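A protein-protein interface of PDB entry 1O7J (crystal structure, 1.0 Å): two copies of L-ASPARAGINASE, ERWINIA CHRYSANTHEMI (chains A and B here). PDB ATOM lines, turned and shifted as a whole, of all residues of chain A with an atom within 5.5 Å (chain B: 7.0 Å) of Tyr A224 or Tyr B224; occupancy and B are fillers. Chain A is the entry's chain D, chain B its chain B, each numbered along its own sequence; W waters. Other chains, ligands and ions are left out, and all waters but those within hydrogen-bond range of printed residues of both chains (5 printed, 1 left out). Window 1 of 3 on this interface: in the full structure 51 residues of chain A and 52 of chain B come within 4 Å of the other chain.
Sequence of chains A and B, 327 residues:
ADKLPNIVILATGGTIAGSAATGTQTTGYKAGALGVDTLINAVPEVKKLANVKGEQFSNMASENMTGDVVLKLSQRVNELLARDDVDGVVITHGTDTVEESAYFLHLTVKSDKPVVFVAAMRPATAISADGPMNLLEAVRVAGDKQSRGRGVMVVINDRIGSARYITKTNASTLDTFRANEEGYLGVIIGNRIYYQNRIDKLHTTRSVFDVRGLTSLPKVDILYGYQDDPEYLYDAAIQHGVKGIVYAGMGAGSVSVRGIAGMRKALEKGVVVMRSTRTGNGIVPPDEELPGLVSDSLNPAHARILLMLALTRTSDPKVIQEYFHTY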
ATOM      1  N   ILE A 222     -12.362  18.798 -29.107  1.00  0.00           N
ATOM      2  CA  ILE A 222     -11.547  19.627 -28.246  1.00  0.00           C
ATOM      3  C   ILE A 222     -10.063  19.230 -28.453  1.00  0.00           C
ATOM      4  O   ILE A 222      -9.752  18.042 -28.314  1.00  0.00           O
ATOM      5  CB  ILE A 222     -11.930  19.496 -26.745  1.00  0.00           C
ATOM      6  CG1 ILE A 222     -13.408  19.814 -26.512  1.00  0.00           C
ATOM      7  CG2 ILE A 222     -11.024  20.355 -25.885  1.00  0.00           C
ATOM      8  CD1 ILE A 222     -13.924  19.587 -25.100  1.00  0.00           C
ATOM      9  N   LEU A 223      -9.225  20.197 -28.762  1.00  0.00           N
ATOM     10  CA  LEU A 223      -7.780  20.049 -28.940  1.00  0.00           C
ATOM     11  C   LEU A 223      -7.061  20.824 -27.866  1.00  0.00           C
ATOM     12  O   LEU A 223      -7.391  21.967 -27.566  1.00  0.00           O
ATOM     13  CB  LEU A 223      -7.317  20.471 -30.324  1.00  0.00           C
ATOM     14  CG  LEU A 223      -7.918  19.709 -31.498  1.00  0.00           C
ATOM     15  CD1 LEU A 223      -7.360  20.229 -32.820  1.00  0.00           C
ATOM     16  CD2 LEU A 223      -7.686  18.207 -31.371  1.00  0.00           C
ATOM     17  N   TYR A 224      -6.056  20.192 -27.273  1.00  0.00           N
ATOM     18  CA  TYR A 224      -5.259  20.804 -26.188  1.00  0.00           C
ATOM     19  C   TYR A 224      -4.144  21.687 -26.724  1.00  0.00           C
ATOM     20  O   TYR A 224      -3.592  21.463 -27.796  1.00  0.00           O
ATOM     21  CB  TYR A 224      -4.671  19.698 -25.309  1.00  0.00           C
ATOM     22  CG  TYR A 224      -4.512  20.003 -23.836  1.00  0.00           C
ATOM     23  CD1 TYR A 224      -5.637  20.145 -23.043  1.00  0.00           C
ATOM     24  CD2 TYR A 224      -3.266  20.103 -23.246  1.00  0.00           C
ATOM     25  CE1 TYR A 224      -5.567  20.412 -21.693  1.00  0.00           C
ATOM     26  CE2 TYR A 224      -3.172  20.322 -21.874  1.00  0.00           C
ATOM     27  CZ  TYR A 224      -4.322  20.456 -21.116  1.00  0.00           C
ATOM     28  OH  TYR A 224      -4.197  20.680 -19.736  1.00  0.00           O
ATOM     29  N   GLY A 225      -3.777  22.699 -25.909  1.00  0.00           N
ATOM     30  CA  GLY A 225      -2.636  23.572 -26.185  1.00  0.00           C
ATOM     31  C   GLY A 225      -1.503  23.338 -25.203  1.00  0.00           C
ATOM     32  O   GLY A 225      -1.736  23.224 -24.009  1.00  0.00           O
ATOM     33  N   TYR A 226      -0.263  23.232 -25.720  1.00  0.00           N
ATOM     34  CA  TYR A 226       0.911  22.847 -24.924  1.00  0.00           C
ATOM     35  C   TYR A 226       2.143  23.061 -25.803  1.00  0.00           C
ATOM     36  O   TYR A 226       2.046  23.206 -27.025  1.00  0.00           O
ATOM     37  CB  TYR A 226       0.809  21.392 -24.449  1.00  0.00           C
ATOM     38  CG  TYR A 226       0.545  20.349 -25.511  1.00  0.00           C
ATOM     39  CD1 TYR A 226      -0.739  20.135 -26.026  1.00  0.00           C
ATOM     40  CD2 TYR A 226       1.585  19.545 -25.995  1.00  0.00           C
ATOM     41  CE1 TYR A 226      -0.976  19.176 -27.007  1.00  0.00           C
ATOM     42  CE2 TYR A 226       1.321  18.555 -26.930  1.00  0.00           C
ATOM     43  CZ  TYR A 226       0.063  18.372 -27.436  1.00  0.00           C
ATOM     44  OH  TYR A 226      -0.242  17.359 -28.334  1.00  0.00           O
ATOM     45  N   ASP A 229       2.722  21.484 -29.489  1.00  0.00           N
ATOM     46  CA  ASP A 229       1.473  20.992 -29.971  1.00  0.00           C
ATOM     47  C   ASP A 229       1.450  20.829 -31.492  1.00  0.00           C
ATOM     48  O   ASP A 229       1.949  21.673 -32.228  1.00  0.00           O
ATOM     49  CB  ASP A 229       0.303  21.867 -29.511  1.00  0.00           C
ATOM     50  CG  ASP A 229       0.344  23.317 -29.911  1.00  0.00           C
ATOM     51  OD1 ASP A 229       1.380  23.912 -30.246  1.00  0.00           O
ATOM     52  OD2 ASP A 229      -0.752  23.883 -29.829  1.00  0.00           O
ATOM     53  N   TYR A 234      -5.238  19.193 -35.925  1.00  0.00           N
ATOM     54  CA  TYR A 234      -6.206  20.023 -36.645  1.00  0.00           C
ATOM     55  C   TYR A 234      -6.569  19.375 -37.986  1.00  0.00           C
ATOM     56  O   TYR A 234      -7.747  19.321 -38.354  1.00  0.00           O
ATOM     57  CB  TYR A 234      -5.670  21.471 -36.887  1.00  0.00           C
ATOM     58  CG  TYR A 234      -5.483  22.207 -35.577  1.00  0.00           C
ATOM     59  CD1 TYR A 234      -4.310  22.025 -34.809  1.00  0.00           C
ATOM     60  CD2 TYR A 234      -6.489  23.030 -35.069  1.00  0.00           C
ATOM     61  CE1 TYR A 234      -4.142  22.689 -33.595  1.00  0.00           C
ATOM     62  CE2 TYR A 234      -6.322  23.673 -33.844  1.00  0.00           C
ATOM     63  CZ  TYR A 234      -5.174  23.501 -33.112  1.00  0.00           C
ATOM     64  OH  TYR A 234      -5.083  24.128 -31.882  1.00  0.00           O
ATOM     65  N   TYR A 247     -10.540  24.873 -28.525  1.00  0.00           N
ATOM     66  CA  TYR A 247      -9.129  24.837 -28.223  1.00  0.00           C
ATOM     67  C   TYR A 247      -8.945  25.099 -26.742  1.00  0.00           C
ATOM     68  O   TYR A 247      -9.299  26.159 -26.227  1.00  0.00           O
ATOM     69  CB  TYR A 247      -8.423  25.876 -29.102  1.00  0.00           C
ATOM     70  CG  TYR A 247      -6.969  26.159 -28.764  1.00  0.00           C
ATOM     71  CD1 TYR A 247      -6.014  25.136 -28.846  1.00  0.00           C
ATOM     72  CD2 TYR A 247      -6.581  27.420 -28.360  1.00  0.00           C
ATOM     73  CE1 TYR A 247      -4.698  25.418 -28.548  1.00  0.00           C
ATOM     74  CE2 TYR A 247      -5.256  27.687 -28.072  1.00  0.00           C
ATOM     75  CZ  TYR A 247      -4.298  26.681 -28.166  1.00  0.00           C
ATOM     76  OH  TYR A 247      -2.988  26.881 -27.830  1.00  0.00           O
ATOM     77  N   ALA A 248      -8.412  24.104 -26.019  1.00  0.00           N
ATOM     78  CA  ALA A 248      -8.118  24.233 -24.589  1.00  0.00           C
ATOM     79  C   ALA A 248      -6.727  24.845 -24.484  1.00  0.00           C
ATOM     80  O   ALA A 248      -5.710  24.179 -24.326  1.00  0.00           O
ATOM     81  CB  ALA A 248      -8.231  22.858 -23.885  1.00  0.00           C
ATOM     82  N   ARG A 278      -6.897  25.907 -21.042  1.00  0.00           N
ATOM     83  CA  ARG A 278      -6.627  24.711 -20.231  1.00  0.00           C
ATOM     84  C   ARG A 278      -6.461  25.019 -18.769  1.00  0.00           C
ATOM     85  O   ARG A 278      -6.341  24.096 -17.921  1.00  0.00           O
ATOM     86  CB  ARG A 278      -5.305  24.024 -20.726  1.00  0.00           C
ATOM     87  CG  ARG A 278      -4.026  24.743 -20.324  1.00  0.00           C
ATOM     88  CD  ARG A 278      -2.763  24.072 -20.893  1.00  0.00           C
ATOM     89  NE  ARG A 278      -1.607  24.609 -20.171  1.00  0.00           N
ATOM     90  CZ  ARG A 278      -0.365  24.383 -20.474  1.00  0.00           C
ATOM     91  NH1 ARG A 278      -0.085  23.677 -21.565  1.00  0.00           N
ATOM     92  NH2 ARG A 278       0.653  24.858 -19.752  1.00  0.00           N
ATOM     93  N   PRO A 300     -13.310  24.360 -21.376  1.00  0.00           N
ATOM     94  CA  PRO A 300     -13.438  23.644 -22.653  1.00  0.00           C
ATOM     95  C   PRO A 300     -14.684  22.778 -22.723  1.00  0.00           C
ATOM     96  O   PRO A 300     -15.359  22.736 -23.769  1.00  0.00           O
ATOM     97  CB  PRO A 300     -12.131  22.859 -22.749  1.00  0.00           C
ATOM     98  CG  PRO A 300     -11.132  23.750 -22.031  1.00  0.00           C
ATOM     99  CD  PRO A 300     -11.926  24.275 -20.849  1.00  0.00           C
ATOM    100  N   ALA A 301     -14.989  22.029 -21.664  1.00  0.00           N
ATOM    101  CA  ALA A 301     -16.146  21.127 -21.680  1.00  0.00           C
ATOM    102  C   ALA A 301     -17.440  21.878 -21.855  1.00  0.00           C
ATOM    103  O   ALA A 301     -18.328  21.482 -22.620  1.00  0.00           O
ATOM    104  CB  ALA A 301     -16.169  20.304 -20.394  1.00  0.00           C
ATOM    105  N   ILE B 222      -0.917  15.278 -26.184  1.00  0.00           N
ATOM    106  CA  ILE B 222      -1.965  15.329 -25.145  1.00  0.00           C
ATOM    107  C   ILE B 222      -3.320  15.316 -25.827  1.00  0.00           C
ATOM    108  O   ILE B 222      -3.561  16.172 -26.690  1.00  0.00           O
ATOM    109  CB  ILE B 222      -1.858  16.539 -24.204  1.00  0.00           C
ATOM    110  CG1 ILE B 222      -0.488  16.624 -23.515  1.00  0.00           C
ATOM    111  CG2 ILE B 222      -3.006  16.538 -23.222  1.00  0.00           C
ATOM    112  CD1 ILE B 222      -0.205  17.884 -22.778  1.00  0.00           C
ATOM    113  N   LEU B 223      -4.158  14.364 -25.452  1.00  0.00           N
ATOM    114  CA  LEU B 223      -5.534  14.229 -25.967  1.00  0.00           C
ATOM    115  C   LEU B 223      -6.533  14.434 -24.855  1.00  0.00           C
ATOM    116  O   LEU B 223      -6.389  13.897 -23.737  1.00  0.00           O
ATOM    117  CB  LEU B 223      -5.743  12.860 -26.601  1.00  0.00           C
ATOM    118  CG  LEU B 223      -4.839  12.561 -27.824  1.00  0.00           C
ATOM    119  CD1 LEU B 223      -5.160  11.184 -28.389  1.00  0.00           C
ATOM    120  CD2 LEU B 223      -4.963  13.617 -28.922  1.00  0.00           C
ATOM    121  N   TYR B 224      -7.588  15.229 -25.107  1.00  0.00           N
ATOM    122  CA  TYR B 224      -8.609  15.565 -24.131  1.00  0.00           C
ATOM    123  C   TYR B 224      -9.698  14.493 -23.987  1.00  0.00           C
ATOM    124  O   TYR B 224     -10.013  13.796 -24.960  1.00  0.00           O
ATOM    125  CB  TYR B 224      -9.244  16.907 -24.507  1.00  0.00           C
ATOM    126  CG  TYR B 224      -9.702  17.790 -23.375  1.00  0.00           C
ATOM    127  CD1 TYR B 224      -8.769  18.374 -22.541  1.00  0.00           C
ATOM    128  CD2 TYR B 224     -11.021  18.091 -23.127  1.00  0.00           C
ATOM    129  CE1 TYR B 224      -9.148  19.188 -21.522  1.00  0.00           C
ATOM    130  CE2 TYR B 224     -11.435  18.936 -22.111  1.00  0.00           C
ATOM    131  CZ  TYR B 224     -10.465  19.509 -21.302  1.00  0.00           C
ATOM    132  OH  TYR B 224     -10.874  20.353 -20.290  1.00  0.00           O
ATOM    133  N   GLY B 225     -10.295  14.389 -22.812  1.00  0.00           N
ATOM    134  CA  GLY B 225     -11.421  13.530 -22.520  1.00  0.00           C
ATOM    135  C   GLY B 225     -12.694  14.333 -22.269  1.00  0.00           C
ATOM    136  O   GLY B 225     -12.676  15.324 -21.556  1.00  0.00           O
ATOM    137  N   TYR B 226     -13.778  13.914 -22.927  1.00  0.00           N
ATOM    138  CA  TYR B 226     -15.043  14.652 -22.886  1.00  0.00           C
ATOM    139  C   TYR B 226     -16.133  13.736 -23.478  1.00  0.00           C
ATOM    140  O   TYR B 226     -15.819  12.730 -24.168  1.00  0.00           O
ATOM    141  CB  TYR B 226     -14.939  15.936 -23.662  1.00  0.00           C
ATOM    142  CG  TYR B 226     -14.396  15.867 -25.092  1.00  0.00           C
ATOM    143  CD1 TYR B 226     -13.042  15.747 -25.358  1.00  0.00           C
ATOM    144  CD2 TYR B 226     -15.259  15.904 -26.186  1.00  0.00           C
ATOM    145  CE1 TYR B 226     -12.540  15.671 -26.639  1.00  0.00           C
ATOM    146  CE2 TYR B 226     -14.775  15.872 -27.497  1.00  0.00           C
ATOM    147  CZ  TYR B 226     -13.419  15.749 -27.711  1.00  0.00           C
ATOM    148  OH  TYR B 226     -12.868  15.760 -28.987  1.00  0.00           O
ATOM    149  N   ASP B 229     -15.926  11.940 -27.128  1.00  0.00           N
ATOM    150  CA  ASP B 229     -14.522  12.044 -27.552  1.00  0.00           C
ATOM    151  C   ASP B 229     -14.211  10.999 -28.654  1.00  0.00           C
ATOM    152  O   ASP B 229     -14.628   9.826 -28.527  1.00  0.00           O
ATOM    153  CB  ASP B 229     -13.581  11.922 -26.406  1.00  0.00           C
ATOM    154  CG  ASP B 229     -13.687  10.716 -25.525  1.00  0.00           C
ATOM    155  OD1 ASP B 229     -14.654   9.948 -25.502  1.00  0.00           O
ATOM    156  OD2 ASP B 229     -12.711  10.529 -24.796  1.00  0.00           O
ATOM    157  N   PRO B 230     -13.463  11.348 -29.669  1.00  0.00           N
ATOM    158  CA  PRO B 230     -13.299  10.444 -30.812  1.00  0.00           C
ATOM    159  C   PRO B 230     -12.094   9.554 -30.801  1.00  0.00           C
ATOM    160  O   PRO B 230     -10.995   9.892 -30.402  1.00  0.00           O
ATOM    161  CB  PRO B 230     -13.147  11.425 -31.980  1.00  0.00           C
ATOM    162  CG  PRO B 230     -12.398  12.589 -31.389  1.00  0.00           C
ATOM    163  CD  PRO B 230     -13.063  12.731 -30.010  1.00  0.00           C
ATOM    164  N   LEU B 233      -8.519  10.654 -33.107  1.00  0.00           N
ATOM    165  CA  LEU B 233      -7.358  11.446 -32.648  1.00  0.00           C
ATOM    166  C   LEU B 233      -6.255  10.546 -32.137  1.00  0.00           C
ATOM    167  O   LEU B 233      -5.092  10.880 -32.302  1.00  0.00           O
ATOM    168  CB  LEU B 233      -7.827  12.482 -31.583  1.00  0.00           C
ATOM    169  CG  LEU B 233      -8.678  13.617 -32.134  1.00  0.00           C
ATOM    170  CD1 LEU B 233      -9.270  14.478 -30.997  1.00  0.00           C
ATOM    171  CD2 LEU B 233      -7.906  14.501 -33.110  1.00  0.00           C
ATOM    172  N   TYR B 234      -6.608   9.412 -31.521  1.00  0.00           N
ATOM    173  CA  TYR B 234      -5.595   8.398 -31.151  1.00  0.00           C
ATOM    174  C   TYR B 234      -4.895   7.846 -32.383  1.00  0.00           C
ATOM    175  O   TYR B 234      -3.679   7.749 -32.466  1.00  0.00           O
ATOM    176  CB  TYR B 234      -6.225   7.252 -30.319  1.00  0.00           C
ATOM    177  CG  TYR B 234      -6.701   7.697 -28.955  1.00  0.00           C
ATOM    178  CD1 TYR B 234      -7.974   8.284 -28.798  1.00  0.00           C
ATOM    179  CD2 TYR B 234      -5.936   7.604 -27.832  1.00  0.00           C
ATOM    180  CE1 TYR B 234      -8.458   8.716 -27.575  1.00  0.00           C
ATOM    181  CE2 TYR B 234      -6.387   8.074 -26.577  1.00  0.00           C
ATOM    182  CZ  TYR B 234      -7.664   8.623 -26.486  1.00  0.00           C
ATOM    183  OH  TYR B 234      -8.054   9.099 -25.228  1.00  0.00           O
ATOM    184  N   VAL B 246      -0.449  11.422 -23.444  1.00  0.00           N
ATOM    185  CA  VAL B 246      -1.025  11.831 -22.163  1.00  0.00           C
ATOM    186  C   VAL B 246      -2.507  12.133 -22.407  1.00  0.00           C
ATOM    187  O   VAL B 246      -2.828  12.914 -23.305  1.00  0.00           O
ATOM    188  CB  VAL B 246      -0.289  13.025 -21.550  1.00  0.00           C
ATOM    189  CG1 VAL B 246      -1.042  13.601 -20.363  1.00  0.00           C
ATOM    190  CG2 VAL B 246       1.118  12.643 -21.160  1.00  0.00           C
ATOM    191  N   TYR B 247      -3.363  11.530 -21.615  1.00  0.00           N
ATOM    192  CA  TYR B 247      -4.816  11.676 -21.697  1.00  0.00           C
ATOM    193  C   TYR B 247      -5.284  12.610 -20.587  1.00  0.00           C
ATOM    194  O   TYR B 247      -5.132  12.321 -19.397  1.00  0.00           O
ATOM    195  CB  TYR B 247      -5.450  10.312 -21.597  1.00  0.00           C
ATOM    196  CG  TYR B 247      -6.951  10.274 -21.382  1.00  0.00           C
ATOM    197  CD1 TYR B 247      -7.768  10.747 -22.355  1.00  0.00           C
ATOM    198  CD2 TYR B 247      -7.522   9.702 -20.244  1.00  0.00           C
ATOM    199  CE1 TYR B 247      -9.172  10.704 -22.228  1.00  0.00           C
ATOM    200  CE2 TYR B 247      -8.914   9.616 -20.079  1.00  0.00           C
ATOM    201  CZ  TYR B 247      -9.702  10.121 -21.093  1.00  0.00           C
ATOM    202  OH  TYR B 247     -11.088  10.135 -20.976  1.00  0.00           O
ATOM    203  N   ALA B 248      -5.848  13.769 -20.959  1.00  0.00           N
ATOM    204  CA  ALA B 248      -6.409  14.728 -20.010  1.00  0.00           C
ATOM    205  C   ALA B 248      -7.845  14.288 -19.738  1.00  0.00           C
ATOM    206  O   ALA B 248      -8.817  14.772 -20.328  1.00  0.00           O
ATOM    207  CB  ALA B 248      -6.322  16.130 -20.583  1.00  0.00           C
ATOM    208  N   GLY B 249      -7.971  13.293 -18.828  1.00  0.00           N
ATOM    209  CA  GLY B 249      -9.162  12.514 -18.720  1.00  0.00           C
ATOM    210  C   GLY B 249     -10.318  13.139 -18.002  1.00  0.00           C
ATOM    211  O   GLY B 249     -10.223  14.075 -17.212  1.00  0.00           O
ATOM    212  N   MET B 250     -11.509  12.594 -18.263  1.00  0.00           N
ATOM    213  CA  MET B 250     -12.695  12.852 -17.459  1.00  0.00           C
ATOM    214  C   MET B 250     -12.465  12.375 -16.010  1.00  0.00           C
ATOM    215  O   MET B 250     -12.013  11.274 -15.830  1.00  0.00           O
ATOM    216  CB  MET B 250     -13.898  12.167 -18.110  1.00  0.00           C
ATOM    217  CG  MET B 250     -14.271  12.782 -19.433  1.00  0.00           C
ATOM    218  SD  MET B 250     -15.520  11.903 -20.370  1.00  0.00           S
ATOM    219  CE  MET B 250     -14.511  10.682 -21.177  1.00  0.00           C
ATOM    220  N   THR B 277      -5.808  13.885 -15.868  1.00  0.00           N
ATOM    221  CA  THR B 277      -7.145  14.415 -15.630  1.00  0.00           C
ATOM    222  C   THR B 277      -7.234  15.829 -16.168  1.00  0.00           C
ATOM    223  O   THR B 277      -6.292  16.627 -16.052  1.00  0.00           O
ATOM    224  CB  THR B 277      -7.506  14.386 -14.106  1.00  0.00           C
ATOM    225  OG1 THR B 277      -8.823  14.933 -13.918  1.00  0.00           O
ATOM    226  CG2 THR B 277      -6.542  15.129 -13.228  1.00  0.00           C
ATOM    227  N   ARG B 278      -8.391  16.166 -16.728  1.00  0.00           N
ATOM    228  CA  ARG B 278      -8.722  17.538 -17.138  1.00  0.00           C
ATOM    229  C   ARG B 278      -9.194  18.394 -15.976  1.00  0.00           C
ATOM    230  O   ARG B 278      -9.407  19.612 -16.176  1.00  0.00           O
ATOM    231  CB  ARG B 278      -9.867  17.503 -18.213  1.00  0.00           C
ATOM    232  CG  ARG B 278     -11.253  17.229 -17.616  1.00  0.00           C
ATOM    233  CD  ARG B 278     -12.298  17.165 -18.750  1.00  0.00           C
ATOM    234  NE  ARG B 278     -13.643  17.218 -18.076  1.00  0.00           N
ATOM    235  CZ  ARG B 278     -14.800  17.013 -18.646  1.00  0.00           C
ATOM    236  NH1 ARG B 278     -14.791  16.683 -19.948  1.00  0.00           N
ATOM    237  NH2 ARG B 278     -15.947  17.114 -18.034  1.00  0.00           N
ATOM    238  N   THR B 279      -9.417  17.811 -14.799  1.00  0.00           N
ATOM    239  CA  THR B 279     -10.161  18.526 -13.754  1.00  0.00           C
ATOM    240  C   THR B 279      -9.375  19.731 -13.215  1.00  0.00           C
ATOM    241  O   THR B 279     -10.011  20.749 -12.840  1.00  0.00           O
ATOM    242  CB  THR B 279     -10.528  17.583 -12.606  1.00  0.00           C
ATOM    243  OG1 THR B 279      -9.351  17.023 -12.014  1.00  0.00           O
ATOM    244  CG2 THR B 279     -11.511  16.509 -13.019  1.00  0.00           C
ATOM    245  N   ASN B 299      -0.682  17.044 -13.504  1.00  0.00           N
ATOM    246  CA  ASN B 299      -1.657  17.502 -14.483  1.00  0.00           C
ATOM    247  C   ASN B 299      -1.124  17.189 -15.904  1.00  0.00           C
ATOM    248  O   ASN B 299      -0.005  16.686 -16.082  1.00  0.00           O
ATOM    249  CB  ASN B 299      -1.970  19.006 -14.286  1.00  0.00           C
ATOM    250  CG  ASN B 299      -0.929  19.969 -14.771  1.00  0.00           C
ATOM    251  OD1 ASN B 299       0.134  19.620 -15.277  1.00  0.00           O
ATOM    252  ND2 ASN B 299      -1.227  21.265 -14.593  1.00  0.00           N
ATOM    253  N   PRO B 300      -1.942  17.409 -16.941  1.00  0.00           N
ATOM    254  CA  PRO B 300      -1.504  16.953 -18.292  1.00  0.00           C
ATOM    255  C   PRO B 300      -0.190  17.551 -18.765  1.00  0.00           C
ATOM    256  O   PRO B 300       0.660  16.855 -19.337  1.00  0.00           O
ATOM    257  CB  PRO B 300      -2.722  17.277 -19.150  1.00  0.00           C
ATOM    258  CG  PRO B 300      -3.895  17.140 -18.198  1.00  0.00           C
ATOM    259  CD  PRO B 300      -3.380  17.731 -16.927  1.00  0.00           C
ATOM    260  N   ALA B 301      -0.021  18.878 -18.568  1.00  0.00           N
ATOM    261  CA  ALA B 301       1.182  19.543 -19.074  1.00  0.00           C
ATOM    262  C   ALA B 301       2.429  18.996 -18.382  1.00  0.00           C
ATOM    263  O   ALA B 301       3.471  18.751 -19.015  1.00  0.00           O
ATOM    264  CB  ALA B 301       1.092  21.045 -18.864  1.00  0.00           C
HETATM  265  O   HOH W   1      -8.019  22.541 -15.594  1.00  0.00           O
HETATM  266  O   HOH W   2      -5.387  17.523 -28.188  1.00  0.00           O
HETATM  267  O   HOH W   3      -2.150  20.761 -17.889  1.00  0.00           O
HETATM  268  O   HOH W   4     -13.208  21.482 -19.415  1.00  0.00           O
HETATM  269  O   HOH W   5      -7.830  16.184 -27.866  1.00  0.00           O
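The side-chain hydroxyl (OH) of Tyr A226 sits at hydrogen-bond distance from the backbone NH (N) of Ile B222.
The side-chain hydroxyl (OH) of Tyr B226 sits at hydrogen-bond distance from the backbone NH (N) of Ile A222 (3.1 Å).
The backbone NH of Tyr B226 lies close to the side-chain sulfur of Met B250 (3.7 Å).
N of Ala B301 lies close to OD1 of Asn B299, at 3.4 Å.
The guanidinium group (NH1) of Arg A278 is in hydrogen-bond range of the backbone carbonyl oxygen (O) of Gly A225 (3.0 Å).
NH1 of Arg B278 lies within hydrogen-bond range of O of Gly B225, at 3.0 Å.
O of Gly B249 is in hydrogen-bond range of N of Arg B278 (2.8 Å).
CD2 of Tyr B224 touches CG2 of Ile A222 (3.6 Å).
CD2 of Tyr A224 touches CG2 of Ile B222, at 3.6 Å.
Tyr A224 touches Tyr B224 (CD1 to CD1, 3.6 Å).
Tyr A224 touches Pro B300 (OH to CB, 3.8 Å).
Ala B301 touches Arg A278 (CB to NH2, 3.9 Å).
Pro A300 touches Tyr B224 (CB to OH, 3.7 Å).
Ala A301 touches Arg B278.
Tyr A224 touches three residues of chain B.
Tyr B224 touches three residues of chain A.
Of the printed residues of chain B, Tyr A226 touches Ile B222.
Of the printed residues of chain B, Pro A300 touches Tyr B224 (3.7 Å).
Of the printed residues of chain B, Ala A301 touches Arg B278.
Of the printed residues of chain A, Pro B300 touches Tyr A224 (3.8 Å).
Of the printed residues of chain A, Arg B278 touches Ala A301.
Tyr B247 touches none of the printed residues of chain A.
Tyr A234 touches none of the printed residues of chain B.
The nearest residue of chain B that does not touch Tyr A224 is Ala B248 (4.5 Å).
The nearest residue of chain A that does not touch Tyr B224 is Ala A248 (4.5 Å).
Of the 20 printed residues of chain B, 6 touch a printed residue of chain A.
Printed residues of chain B that touch a printed residue of chain A: Ile B222, Tyr B224, Tyr B226, Arg B278, Pro B300 and Ala B301.
Hydrophobic or aromatic side chains of chain B that line the printed part of chain A: Ile B222, Tyr B224, Tyr B226, Pro B300 and Ala B301.
Of the 12 printed residues of chain A, 6 touch a printed residue of chain B.
Among the printed residues, no Asp or Glu carboxylate lies within 4 Å of a Lys or Arg side-chain nitrogen of the other chain.
Ile A222 touches Tyr B224, and with the chains exchanged Tyr A224 touches Ile B222.
Ile A222 touches Tyr B226, and with the chains exchanged Tyr A226 touches Ile B222.
Tyr B224 touches its own counterpart, Tyr A224.
Arg A278 touches Ala B301, and with the chains exchanged Ala A301 touches Arg B278.
Of the 9 pairs that touch across the chains among the printed residues, 9 have their exchanged pair printed and touching as well.
Water W5 lies within hydrogen-bond range of O of Ile A222 (2.7 Å) and N of Tyr B224 (2.9 Å).
Water W2 lies within hydrogen-bond range of O of Ile B222 (2.7 Å) and N of Tyr A224 (2.9 Å).
Water W4 lies within hydrogen-bond range of the side-chain hydroxyl (OH) of Tyr B224 (2.7 Å) and the backbone NH (N) of Ala A301 (2.9 Å).
Water W3 lies within hydrogen-bond range of the side-chain hydroxyl (OH) of Tyr A224 (2.8 Å), the backbone NH (N) of Ala B301 (2.9 Å) and the side-chain amide nitrogen (ND2) of Asn B299 (3.5 Å).
Water W1 bridges the backbone carbonyl oxygen (O) of Arg A278 (3.3 Å) and the backbone carbonyl oxygen (O) of Arg B278 (3.3 Å).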
